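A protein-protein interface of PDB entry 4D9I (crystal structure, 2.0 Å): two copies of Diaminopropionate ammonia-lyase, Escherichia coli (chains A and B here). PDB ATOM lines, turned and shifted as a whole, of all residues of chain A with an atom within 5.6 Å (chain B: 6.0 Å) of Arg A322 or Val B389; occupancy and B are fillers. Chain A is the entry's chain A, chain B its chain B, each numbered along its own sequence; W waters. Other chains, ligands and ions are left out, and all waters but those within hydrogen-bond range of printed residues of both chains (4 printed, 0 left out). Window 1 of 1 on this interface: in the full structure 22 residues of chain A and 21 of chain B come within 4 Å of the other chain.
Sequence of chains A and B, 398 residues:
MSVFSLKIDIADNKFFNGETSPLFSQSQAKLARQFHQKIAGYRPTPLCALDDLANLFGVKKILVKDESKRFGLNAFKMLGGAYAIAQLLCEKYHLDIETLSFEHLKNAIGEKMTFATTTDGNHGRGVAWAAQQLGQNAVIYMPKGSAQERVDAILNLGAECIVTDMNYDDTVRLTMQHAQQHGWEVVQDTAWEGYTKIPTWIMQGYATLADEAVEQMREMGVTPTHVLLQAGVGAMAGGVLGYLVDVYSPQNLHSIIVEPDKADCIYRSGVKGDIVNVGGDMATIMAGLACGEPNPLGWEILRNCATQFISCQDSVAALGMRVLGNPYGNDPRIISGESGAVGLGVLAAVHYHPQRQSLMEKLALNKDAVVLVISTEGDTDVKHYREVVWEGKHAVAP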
ATOM      1  N   SER A 315     -23.707   2.710  -8.054  1.00  0.00           N
ATOM      2  CA  SER A 315     -23.759   2.382  -9.486  1.00  0.00           C
ATOM      3  C   SER A 315     -24.639   1.156  -9.810  1.00  0.00           C
ATOM      4  O   SER A 315     -24.967   0.897 -10.979  1.00  0.00           O
ATOM      5  CB  SER A 315     -22.340   2.219 -10.064  1.00  0.00           C
ATOM      6  OG  SER A 315     -21.741   1.053  -9.561  1.00  0.00           O
ATOM      7  N   ALA A 317     -27.670   1.068  -8.928  1.00  0.00           N
ATOM      8  CA  ALA A 317     -28.921   1.723  -9.342  1.00  0.00           C
ATOM      9  C   ALA A 317     -28.867   2.043 -10.850  1.00  0.00           C
ATOM     10  O   ALA A 317     -29.820   1.772 -11.600  1.00  0.00           O
ATOM     11  CB  ALA A 317     -29.154   2.982  -8.525  1.00  0.00           C
ATOM     12  N   ALA A 318     -27.734   2.584 -11.283  1.00  0.00           N
ATOM     13  CA  ALA A 318     -27.534   2.962 -12.694  1.00  0.00           C
ATOM     14  C   ALA A 318     -27.604   1.764 -13.624  1.00  0.00           C
ATOM     15  O   ALA A 318     -28.109   1.859 -14.750  1.00  0.00           O
ATOM     16  CB  ALA A 318     -26.198   3.676 -12.851  1.00  0.00           C
ATOM     17  N   LEU A 319     -27.040   0.639 -13.173  1.00  0.00           N
ATOM     18  CA  LEU A 319     -27.115  -0.641 -13.911  1.00  0.00           C
ATOM     19  C   LEU A 319     -28.583  -1.048 -14.085  1.00  0.00           C
ATOM     20  O   LEU A 319     -29.024  -1.389 -15.192  1.00  0.00           O
ATOM     21  CB  LEU A 319     -26.377  -1.731 -13.126  1.00  0.00           C
ATOM     22  CG  LEU A 319     -26.362  -3.155 -13.678  1.00  0.00           C
ATOM     23  CD1 LEU A 319     -25.745  -3.181 -15.080  1.00  0.00           C
ATOM     24  CD2 LEU A 319     -25.576  -4.103 -12.747  1.00  0.00           C
ATOM     25  N   GLY A 320     -29.328  -1.004 -12.972  1.00  0.00           N
ATOM     26  CA  GLY A 320     -30.778  -1.250 -12.986  1.00  0.00           C
ATOM     27  C   GLY A 320     -31.528  -0.388 -14.012  1.00  0.00           C
ATOM     28  O   GLY A 320     -32.330  -0.898 -14.800  1.00  0.00           O
ATOM     29  N   MET A 321     -31.268   0.921 -14.013  1.00  0.00           N
ATOM     30  CA  MET A 321     -31.930   1.818 -14.950  1.00  0.00           C
ATOM     31  C   MET A 321     -31.740   1.313 -16.373  1.00  0.00           C
ATOM     32  O   MET A 321     -32.701   1.244 -17.160  1.00  0.00           O
ATOM     33  CB  MET A 321     -31.386   3.243 -14.827  1.00  0.00           C
ATOM     34  CG  MET A 321     -31.638   3.890 -13.473  1.00  0.00           C
ATOM     35  SD  MET A 321     -30.698   5.398 -13.244  1.00  0.00           S
ATOM     36  CE  MET A 321     -31.514   6.541 -14.370  1.00  0.00           C
ATOM     37  N   ARG A 322     -30.508   0.951 -16.713  1.00  0.00           N
ATOM     38  CA  ARG A 322     -30.182   0.607 -18.098  1.00  0.00           C
ATOM     39  C   ARG A 322     -30.816  -0.711 -18.513  1.00  0.00           C
ATOM     40  O   ARG A 322     -31.338  -0.838 -19.621  1.00  0.00           O
ATOM     41  CB  ARG A 322     -28.675   0.603 -18.331  1.00  0.00           C
ATOM     42  CG  ARG A 322     -28.079   1.996 -18.314  1.00  0.00           C
ATOM     43  CD  ARG A 322     -26.618   1.993 -18.721  1.00  0.00           C
ATOM     44  NE  ARG A 322     -25.926   3.057 -18.001  1.00  0.00           N
ATOM     45  CZ  ARG A 322     -25.168   2.862 -16.939  1.00  0.00           C
ATOM     46  NH1 ARG A 322     -24.978   1.656 -16.459  1.00  0.00           N
ATOM     47  NH2 ARG A 322     -24.626   3.895 -16.343  1.00  0.00           N
ATOM     48  N   VAL A 323     -30.791  -1.675 -17.601  1.00  0.00           N
ATOM     49  CA  VAL A 323     -31.372  -2.985 -17.847  1.00  0.00           C
ATOM     50  C   VAL A 323     -32.894  -2.850 -18.055  1.00  0.00           C
ATOM     51  O   VAL A 323     -33.457  -3.452 -18.968  1.00  0.00           O
ATOM     52  CB  VAL A 323     -31.028  -3.980 -16.703  1.00  0.00           C
ATOM     53  CG1 VAL A 323     -31.882  -5.234 -16.805  1.00  0.00           C
ATOM     54  CG2 VAL A 323     -29.534  -4.330 -16.698  1.00  0.00           C
ATOM     55  N   LEU A 324     -33.550  -2.072 -17.217  1.00  0.00           N
ATOM     56  CA  LEU A 324     -34.984  -1.830 -17.383  1.00  0.00           C
ATOM     57  C   LEU A 324     -35.341  -1.097 -18.686  1.00  0.00           C
ATOM     58  O   LEU A 324     -36.320  -1.448 -19.353  1.00  0.00           O
ATOM     59  CB  LEU A 324     -35.580  -1.113 -16.156  1.00  0.00           C
ATOM     60  CG  LEU A 324     -35.771  -2.015 -14.924  1.00  0.00           C
ATOM     61  CD1 LEU A 324     -35.923  -1.202 -13.623  1.00  0.00           C
ATOM     62  CD2 LEU A 324     -36.950  -2.975 -15.075  1.00  0.00           C
ATOM     63  N   GLY A 325     -34.523  -0.101 -19.037  1.00  0.00           N
ATOM     64  CA  GLY A 325     -34.754   0.772 -20.195  1.00  0.00           C
ATOM     65  C   GLY A 325     -34.465   0.129 -21.547  1.00  0.00           C
ATOM     66  O   GLY A 325     -34.959   0.582 -22.571  1.00  0.00           O
ATOM     67  N   ASN A 326     -33.650  -0.913 -21.563  1.00  0.00           N
ATOM     68  CA  ASN A 326     -33.369  -1.631 -22.803  1.00  0.00           C
ATOM     69  C   ASN A 326     -33.412  -3.111 -22.463  1.00  0.00           C
ATOM     70  O   ASN A 326     -32.370  -3.697 -22.187  1.00  0.00           O
ATOM     71  CB  ASN A 326     -31.981  -1.263 -23.343  1.00  0.00           C
ATOM     72  CG  ASN A 326     -31.697  -1.875 -24.708  1.00  0.00           C
ATOM     73  OD1 ASN A 326     -32.360  -2.804 -25.138  1.00  0.00           O
ATOM     74  ND2 ASN A 326     -30.698  -1.341 -25.390  1.00  0.00           N
ATOM     75  N   PRO A 327     -34.621  -3.701 -22.464  1.00  0.00           N
ATOM     76  CA  PRO A 327     -34.799  -5.041 -21.920  1.00  0.00           C
ATOM     77  C   PRO A 327     -34.166  -6.155 -22.782  1.00  0.00           C
ATOM     78  O   PRO A 327     -33.836  -5.965 -23.968  1.00  0.00           O
ATOM     79  CB  PRO A 327     -36.319  -5.180 -21.844  1.00  0.00           C
ATOM     80  CG  PRO A 327     -36.810  -4.313 -22.953  1.00  0.00           C
ATOM     81  CD  PRO A 327     -35.904  -3.118 -22.907  1.00  0.00           C
ATOM     82  N   VAL A 388     -27.392   8.661 -17.648  1.00  0.00           N
ATOM     83  CA  VAL A 388     -27.242   7.266 -17.294  1.00  0.00           C
ATOM     84  C   VAL A 388     -27.459   6.350 -18.514  1.00  0.00           C
ATOM     85  O   VAL A 388     -26.541   5.626 -18.878  1.00  0.00           O
ATOM     86  CB  VAL A 388     -28.173   6.854 -16.133  1.00  0.00           C
ATOM     87  CG1 VAL A 388     -28.146   5.333 -15.950  1.00  0.00           C
ATOM     88  CG2 VAL A 388     -27.765   7.552 -14.825  1.00  0.00           C
ATOM     89  N   VAL A 389     -28.637   6.395 -19.160  1.00  0.00           N
ATOM     90  CA  VAL A 389     -28.956   5.361 -20.191  1.00  0.00           C
ATOM     91  C   VAL A 389     -28.324   5.565 -21.560  1.00  0.00           C
ATOM     92  O   VAL A 389     -28.092   4.593 -22.314  1.00  0.00           O
ATOM     93  CB  VAL A 389     -30.468   5.092 -20.332  1.00  0.00           C
ATOM     94  CG1 VAL A 389     -31.048   4.747 -18.955  1.00  0.00           C
ATOM     95  CG2 VAL A 389     -31.200   6.277 -20.976  1.00  0.00           C
ATOM     96  N   GLY A 392     -23.959   6.761 -20.487  1.00  0.00           N
ATOM     97  CA  GLY A 392     -23.249   5.739 -19.739  1.00  0.00           C
ATOM     98  C   GLY A 392     -22.623   6.286 -18.466  1.00  0.00           C
ATOM     99  O   GLY A 392     -21.663   5.719 -17.950  1.00  0.00           O
ATOM    100  N   LYS A 393     -23.180   7.382 -17.945  1.00  0.00           N
ATOM    101  CA  LYS A 393     -22.765   7.902 -16.637  1.00  0.00           C
ATOM    102  C   LYS A 393     -22.919   6.825 -15.559  1.00  0.00           C
ATOM    103  O   LYS A 393     -23.806   5.978 -15.650  1.00  0.00           O
ATOM    104  CB  LYS A 393     -23.618   9.117 -16.256  1.00  0.00           C
ATOM    105  CG  LYS A 393     -23.119   9.873 -15.019  1.00  0.00           C
ATOM    106  CD  LYS A 393     -23.908  11.154 -14.785  1.00  0.00           C
ATOM    107  CE  LYS A 393     -25.333  10.863 -14.355  1.00  0.00           C
ATOM    108  NZ  LYS A 393     -25.990  12.098 -13.856  1.00  0.00           N
ATOM    109  N   HIS A 394     -22.085   6.880 -14.522  1.00  0.00           N
ATOM    110  CA  HIS A 394     -22.074   5.836 -13.485  1.00  0.00           C
ATOM    111  C   HIS A 394     -21.957   4.471 -14.096  1.00  0.00           C
ATOM    112  O   HIS A 394     -22.673   3.533 -13.713  1.00  0.00           O
ATOM    113  CB  HIS A 394     -23.303   5.925 -12.570  1.00  0.00           C
ATOM    114  CG  HIS A 394     -23.452   7.258 -11.892  1.00  0.00           C
ATOM    115  ND1 HIS A 394     -24.652   7.781 -11.583  1.00  0.00           N
ATOM    116  CD2 HIS A 394     -22.498   8.194 -11.499  1.00  0.00           C
ATOM    117  CE1 HIS A 394     -24.478   8.978 -10.989  1.00  0.00           C
ATOM    118  NE2 HIS A 394     -23.154   9.234 -10.951  1.00  0.00           N
ATOM    119  N   ALA A 395     -21.050   4.375 -15.068  1.00  0.00           N
ATOM    120  CA  ALA A 395     -20.693   3.129 -15.720  1.00  0.00           C
ATOM    121  C   ALA A 395     -20.269   2.084 -14.707  1.00  0.00           C
ATOM    122  O   ALA A 395     -19.921   2.392 -13.566  1.00  0.00           O
ATOM    123  CB  ALA A 395     -19.578   3.359 -16.733  1.00  0.00           C
ATOM    124  N   VAL A 396     -20.295   0.837 -15.143  1.00  0.00           N
ATOM    125  CA  VAL A 396     -19.978  -0.290 -14.294  1.00  0.00           C
ATOM    126  C   VAL A 396     -18.469  -0.439 -14.025  1.00  0.00           C
ATOM    127  O   VAL A 396     -18.070  -0.681 -12.883  1.00  0.00           O
ATOM    128  CB  VAL A 396     -20.586  -1.562 -14.916  1.00  0.00           C
ATOM    129  CG1 VAL A 396     -19.616  -2.730 -14.885  1.00  0.00           C
ATOM    130  CG2 VAL A 396     -21.919  -1.881 -14.270  1.00  0.00           C
ATOM    131  N   ALA B 318     -20.946   3.707 -29.716  1.00  0.00           N
ATOM    132  CA  ALA B 318     -21.520   3.300 -28.424  1.00  0.00           C
ATOM    133  C   ALA B 318     -22.730   4.166 -28.027  1.00  0.00           C
ATOM    134  O   ALA B 318     -23.764   3.635 -27.655  1.00  0.00           O
ATOM    135  CB  ALA B 318     -20.464   3.312 -27.337  1.00  0.00           C
ATOM    136  N   MET B 321     -25.700   3.223 -30.169  1.00  0.00           N
ATOM    137  CA  MET B 321     -26.291   1.956 -29.734  1.00  0.00           C
ATOM    138  C   MET B 321     -27.296   2.182 -28.589  1.00  0.00           C
ATOM    139  O   MET B 321     -28.404   1.623 -28.599  1.00  0.00           O
ATOM    140  CB  MET B 321     -25.202   1.004 -29.243  1.00  0.00           C
ATOM    141  CG  MET B 321     -24.246   0.516 -30.330  1.00  0.00           C
ATOM    142  SD  MET B 321     -22.815  -0.357 -29.660  1.00  0.00           S
ATOM    143  CE  MET B 321     -23.487  -1.919 -29.108  1.00  0.00           C
ATOM    144  N   ARG B 322     -26.890   2.972 -27.605  1.00  0.00           N
ATOM    145  CA  ARG B 322     -27.738   3.244 -26.434  1.00  0.00           C
ATOM    146  C   ARG B 322     -28.975   4.068 -26.770  1.00  0.00           C
ATOM    147  O   ARG B 322     -30.069   3.829 -26.210  1.00  0.00           O
ATOM    148  CB  ARG B 322     -26.938   3.951 -25.345  1.00  0.00           C
ATOM    149  CG  ARG B 322     -25.836   3.077 -24.748  1.00  0.00           C
ATOM    150  CD  ARG B 322     -25.131   3.783 -23.609  1.00  0.00           C
ATOM    151  NE  ARG B 322     -23.825   3.182 -23.433  1.00  0.00           N
ATOM    152  CZ  ARG B 322     -22.689   3.768 -23.756  1.00  0.00           C
ATOM    153  NH1 ARG B 322     -22.683   5.006 -24.244  1.00  0.00           N
ATOM    154  NH2 ARG B 322     -21.576   3.121 -23.552  1.00  0.00           N
ATOM    155  N   GLY B 325     -31.391   1.892 -28.649  1.00  0.00           N
ATOM    156  CA  GLY B 325     -31.894   0.798 -27.835  1.00  0.00           C
ATOM    157  C   GLY B 325     -32.787   1.248 -26.683  1.00  0.00           C
ATOM    158  O   GLY B 325     -33.505   0.427 -26.099  1.00  0.00           O
ATOM    159  N   ASN B 326     -32.731   2.533 -26.330  1.00  0.00           N
ATOM    160  CA  ASN B 326     -33.614   3.060 -25.296  1.00  0.00           C
ATOM    161  C   ASN B 326     -34.104   4.410 -25.775  1.00  0.00           C
ATOM    162  O   ASN B 326     -33.561   5.447 -25.410  1.00  0.00           O
ATOM    163  CB  ASN B 326     -32.911   3.133 -23.920  1.00  0.00           C
ATOM    164  CG  ASN B 326     -33.822   3.648 -22.811  1.00  0.00           C
ATOM    165  OD1 ASN B 326     -34.954   4.107 -23.058  1.00  0.00           O
ATOM    166  ND2 ASN B 326     -33.308   3.639 -21.581  1.00  0.00           N
ATOM    167  N   HIS B 384     -20.949  -7.905 -26.217  1.00  0.00           N
ATOM    168  CA  HIS B 384     -20.567  -6.506 -26.435  1.00  0.00           C
ATOM    169  C   HIS B 384     -21.762  -5.573 -26.387  1.00  0.00           C
ATOM    170  O   HIS B 384     -21.702  -4.456 -25.814  1.00  0.00           O
ATOM    171  CB  HIS B 384     -19.810  -6.419 -27.769  1.00  0.00           C
ATOM    172  CG  HIS B 384     -19.422  -5.024 -28.168  1.00  0.00           C
ATOM    173  ND1 HIS B 384     -18.413  -4.355 -27.577  1.00  0.00           N
ATOM    174  CD2 HIS B 384     -19.961  -4.167 -29.124  1.00  0.00           C
ATOM    175  CE1 HIS B 384     -18.305  -3.132 -28.126  1.00  0.00           C
ATOM    176  NE2 HIS B 384     -19.256  -3.017 -29.079  1.00  0.00           N
ATOM    177  N   TYR B 385     -22.855  -5.995 -27.023  1.00  0.00           N
ATOM    178  CA  TYR B 385     -24.058  -5.162 -27.080  1.00  0.00           C
ATOM    179  C   TYR B 385     -24.512  -4.819 -25.651  1.00  0.00           C
ATOM    180  O   TYR B 385     -24.745  -3.656 -25.324  1.00  0.00           O
ATOM    181  CB  TYR B 385     -25.197  -5.862 -27.831  1.00  0.00           C
ATOM    182  CG  TYR B 385     -26.422  -4.966 -27.918  1.00  0.00           C
ATOM    183  CD1 TYR B 385     -26.472  -3.926 -28.840  1.00  0.00           C
ATOM    184  CD2 TYR B 385     -27.495  -5.130 -27.038  1.00  0.00           C
ATOM    185  CE1 TYR B 385     -27.568  -3.067 -28.912  1.00  0.00           C
ATOM    186  CE2 TYR B 385     -28.599  -4.288 -27.100  1.00  0.00           C
ATOM    187  CZ  TYR B 385     -28.631  -3.270 -28.013  1.00  0.00           C
ATOM    188  OH  TYR B 385     -29.715  -2.463 -28.072  1.00  0.00           O
ATOM    189  N   ARG B 386     -24.597  -5.845 -24.807  1.00  0.00           N
ATOM    190  CA  ARG B 386     -25.093  -5.652 -23.443  1.00  0.00           C
ATOM    191  C   ARG B 386     -24.071  -4.927 -22.560  1.00  0.00           C
ATOM    192  O   ARG B 386     -24.451  -4.116 -21.694  1.00  0.00           O
ATOM    193  CB  ARG B 386     -25.547  -6.982 -22.828  1.00  0.00           C
ATOM    194  CG  ARG B 386     -26.798  -7.565 -23.488  1.00  0.00           C
ATOM    195  CD  ARG B 386     -27.935  -6.551 -23.565  1.00  0.00           C
ATOM    196  NE  ARG B 386     -29.005  -7.001 -24.457  1.00  0.00           N
ATOM    197  CZ  ARG B 386     -30.214  -6.445 -24.524  1.00  0.00           C
ATOM    198  NH1 ARG B 386     -30.525  -5.407 -23.744  1.00  0.00           N
ATOM    199  NH2 ARG B 386     -31.111  -6.923 -25.385  1.00  0.00           N
ATOM    200  N   GLU B 387     -22.783  -5.187 -22.789  1.00  0.00           N
ATOM    201  CA  GLU B 387     -21.737  -4.405 -22.121  1.00  0.00           C
ATOM    202  C   GLU B 387     -21.881  -2.896 -22.408  1.00  0.00           C
ATOM    203  O   GLU B 387     -21.739  -2.059 -21.500  1.00  0.00           O
ATOM    204  CB  GLU B 387     -20.332  -4.942 -22.480  1.00  0.00           C
ATOM    205  CG  GLU B 387     -19.992  -6.202 -21.717  1.00  0.00           C
ATOM    206  CD  GLU B 387     -18.846  -7.016 -22.313  1.00  0.00           C
ATOM    207  OE1 GLU B 387     -18.314  -6.675 -23.387  1.00  0.00           O
ATOM    208  OE2 GLU B 387     -18.492  -8.025 -21.698  1.00  0.00           O
ATOM    209  N   VAL B 388     -22.219  -2.547 -23.649  1.00  0.00           N
ATOM    210  CA  VAL B 388     -22.451  -1.137 -23.999  1.00  0.00           C
ATOM    211  C   VAL B 388     -23.745  -0.578 -23.374  1.00  0.00           C
ATOM    212  O   VAL B 388     -23.718   0.467 -22.704  1.00  0.00           O
ATOM    213  CB  VAL B 388     -22.443  -0.896 -25.531  1.00  0.00           C
ATOM    214  CG1 VAL B 388     -22.807   0.554 -25.878  1.00  0.00           C
ATOM    215  CG2 VAL B 388     -21.085  -1.251 -26.136  1.00  0.00           C
ATOM    216  N   VAL B 389     -24.873  -1.244 -23.613  1.00  0.00           N
ATOM    217  CA  VAL B 389     -26.187  -0.637 -23.280  1.00  0.00           C
ATOM    218  C   VAL B 389     -26.527  -0.776 -21.798  1.00  0.00           C
ATOM    219  O   VAL B 389     -27.209   0.094 -21.223  1.00  0.00           O
ATOM    220  CB  VAL B 389     -27.347  -1.104 -24.203  1.00  0.00           C
ATOM    221  CG1 VAL B 389     -26.996  -0.843 -25.671  1.00  0.00           C
ATOM    222  CG2 VAL B 389     -27.710  -2.570 -23.995  1.00  0.00           C
ATOM    223  N   TRP B 390     -26.038  -1.851 -21.182  1.00  0.00           N
ATOM    224  CA  TRP B 390     -26.251  -2.088 -19.737  1.00  0.00           C
ATOM    225  C   TRP B 390     -25.101  -1.677 -18.854  1.00  0.00           C
ATOM    226  O   TRP B 390     -25.299  -1.013 -17.832  1.00  0.00           O
ATOM    227  CB  TRP B 390     -26.553  -3.558 -19.473  1.00  0.00           C
ATOM    228  CG  TRP B 390     -27.889  -4.068 -19.975  1.00  0.00           C
ATOM    229  CD1 TRP B 390     -28.933  -3.342 -20.543  1.00  0.00           C
ATOM    230  CD2 TRP B 390     -28.379  -5.460 -19.923  1.00  0.00           C
ATOM    231  NE1 TRP B 390     -29.985  -4.164 -20.849  1.00  0.00           N
ATOM    232  CE2 TRP B 390     -29.729  -5.442 -20.489  1.00  0.00           C
ATOM    233  CE3 TRP B 390     -27.852  -6.672 -19.474  1.00  0.00           C
ATOM    234  CZ2 TRP B 390     -30.496  -6.602 -20.602  1.00  0.00           C
ATOM    235  CZ3 TRP B 390     -28.636  -7.830 -19.598  1.00  0.00           C
ATOM    236  CH2 TRP B 390     -29.922  -7.791 -20.149  1.00  0.00           C
ATOM    237  N   GLU B 391     -23.878  -2.077 -19.213  1.00  0.00           N
ATOM    238  CA  GLU B 391     -22.717  -1.840 -18.333  1.00  0.00           C
ATOM    239  C   GLU B 391     -22.163  -0.430 -18.521  1.00  0.00           C
ATOM    240  O   GLU B 391     -21.400   0.070 -17.695  1.00  0.00           O
ATOM    241  CB  GLU B 391     -21.626  -2.899 -18.557  1.00  0.00           C
ATOM    242  CG  GLU B 391     -22.082  -4.313 -18.229  1.00  0.00           C
ATOM    243  CD  GLU B 391     -21.013  -5.373 -18.420  1.00  0.00           C
ATOM    244  OE1 GLU B 391     -19.805  -5.064 -18.346  1.00  0.00           O
ATOM    245  OE2 GLU B 391     -21.390  -6.542 -18.601  1.00  0.00           O
ATOM    246  N   GLY B 392     -22.563   0.210 -19.610  1.00  0.00           N
ATOM    247  CA  GLY B 392     -22.048   1.530 -19.951  1.00  0.00           C
ATOM    248  C   GLY B 392     -20.601   1.507 -20.437  1.00  0.00           C
ATOM    249  O   GLY B 392     -19.925   2.527 -20.401  1.00  0.00           O
ATOM    250  N   LYS B 393     -20.122   0.338 -20.863  1.00  0.00           N
ATOM    251  CA  LYS B 393     -18.851   0.248 -21.603  1.00  0.00           C
ATOM    252  C   LYS B 393     -18.778   1.298 -22.728  1.00  0.00           C
ATOM    253  O   LYS B 393     -19.781   1.574 -23.410  1.00  0.00           O
ATOM    254  CB  LYS B 393     -18.655  -1.162 -22.189  1.00  0.00           C
ATOM    255  CG  LYS B 393     -17.243  -1.428 -22.698  1.00  0.00           C
ATOM    256  CD  LYS B 393     -17.019  -2.889 -23.100  1.00  0.00           C
ATOM    257  CE  LYS B 393     -17.587  -3.173 -24.493  1.00  0.00           C
ATOM    258  NZ  LYS B 393     -17.445  -4.602 -24.912  1.00  0.00           N
HETATM  259  O   HOH W   1     -31.400   1.554 -21.131  1.00  0.00           O
HETATM  260  O   HOH W   2     -28.545   2.091 -22.121  1.00  0.00           O
HETATM  261  O   HOH W   3     -33.970  -7.069 -27.012  1.00  0.00           O
HETATM  262  O   HOH W   4     -29.928   1.388 -24.817  1.00  0.00           O
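Arg A322 touches Val B389, and with the chains exchanged Val A389 touches Arg B322. Gly A325 touches its own counterpart, Gly B325. Gly A325 touches Asn B326, and with the chains exchanged Asn A326 touches Gly B325. Asn A326 touches Val B389, and with the chains exchanged Val A389 touches Asn B326. Positions printed for both chains: 318, 321, 322, 325, 326, 388, 389, 392 and 393.
Arg A322 touches just these residues of chain B: Val B389 and Trp B390. Of chain A, only Arg A322 (3.2 Å) and Asn A326 (3.5 Å) come within 4 Å of Val B389. Of the printed residues of chain A, Arg B386 touches Asn A326 and Pro A327. Of the printed residues of chain B, Asn A326 touches Gly B325, Tyr B385, Arg B386, Val B389 and Trp B390. Printed residues of chain B within 4 Å of Pro A327: Arg B386. Of the printed residues of chain B, Val A389 touches Arg B322 and Asn B326. Val A388 touches none of the printed residues of chain B. The nearest printed residue of chain A that does not touch Gly B325 is Pro A327 (5.3 Å).
The guanidinium group (NE) of Arg A322 lies within hydrogen-bond range of the backbone carbonyl oxygen (O) of Val A388, at 2.8 Å. The backbone carbonyl oxygen (O) of His A394 is in hydrogen-bond range of the guanidinium group (NH2) of Arg A322, 3.3 Å away. The backbone carbonyl oxygen (O) of Val B388 lies within hydrogen-bond range of the guanidinium group (NE) of Arg B322 (2.8 Å). The backbone NH (N) of Glu B391 lies within hydrogen-bond range of the backbone carbonyl oxygen (O) of Arg B386 (3.3 Å). O of Glu B387 sits at hydrogen-bond distance from N of Gly B392, 3.1 Å away.
The guanidinium group (NH1) of Arg A322 lies within hydrogen-bond range of the backbone carbonyl oxygen (O) of Trp B390, at 3.0 Å. The backbone carbonyl oxygen (O) of Gly B325 lies close to the side-chain amide nitrogen (ND2) of Asn A326 (3.4 Å). ND2 of Asn A326 sits at hydrogen-bond distance from OH of Tyr B385. The guanidinium group of Arg B386 lies within hydrogen-bond range of the backbone carbonyl oxygen of Asn A326 (3.0 Å). NE1 of Trp B390 sits at hydrogen-bond distance from O of Asn A326 (2.8 Å). O of Pro A327 sits at hydrogen-bond distance from NH2 of Arg B386 (3.2 Å). N of Val A396 sits at hydrogen-bond distance from O of Glu B391 (2.9 Å).
Of the 15 printed residues of chain B, 9 touch a printed residue of chain A. Hydrophobic or aromatic side chains of chain B that line the printed part of chain A: Tyr B385, Val B389 and Trp B390. Of the 19 printed residues of chain A, 9 touch a printed residue of chain B. Hydrophobic or aromatic side chains of chain A that line the printed part of chain B: Leu A319, Val A323, Val A389, Ala A395 and Val A396. Along chain A the printed residues that touch a printed residue of chain B span positions 319 to 396. Among the printed residues, 17 pairs touch across the chains. Among the printed residues, no Asp or Glu carboxylate lies within 4 Å of a Lys or Arg side-chain nitrogen of the other chain.
Water W2 lies within hydrogen-bond range of O of Val A389 (2.5 Å) and O of Val B389 (2.6 Å). Water W4 lies within hydrogen-bond range of the backbone carbonyl oxygen of Arg B322 (2.8 Å), the side-chain amide nitrogen of Asn A326 (2.9 Å) and the backbone NH of Asn B326 (3.4 Å). Water W1 lies within hydrogen-bond range of O of Arg A322 (2.8 Å), ND2 of Asn B326 (2.9 Å) and N of Asn A326 (3.4 Å). Water W3 lies within hydrogen-bond range of O of Pro A327 (3.2 Å) and NH2 of Arg B386 (3.3 Å).
Among the printed residues, merely in contact across the chains: Arg A322 with Val B389 (3.2 Å), Gly A325 with Asn B326 (3.3 Å), Val A389 with Arg B322 (3.3 Å), Val A389 with Asn B326 (3.4 Å), Val A323 with Trp B390 (3.5 Å), Asn A326 with Val B389 (3.5 Å), Leu A319 with Trp B390 (3.5 Å), Ala A395 with Glu B391 (3.7 Å), Ala A395 with Gly B392 (3.8 Å) and Gly A325 with Gly B325 (3.8 Å).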
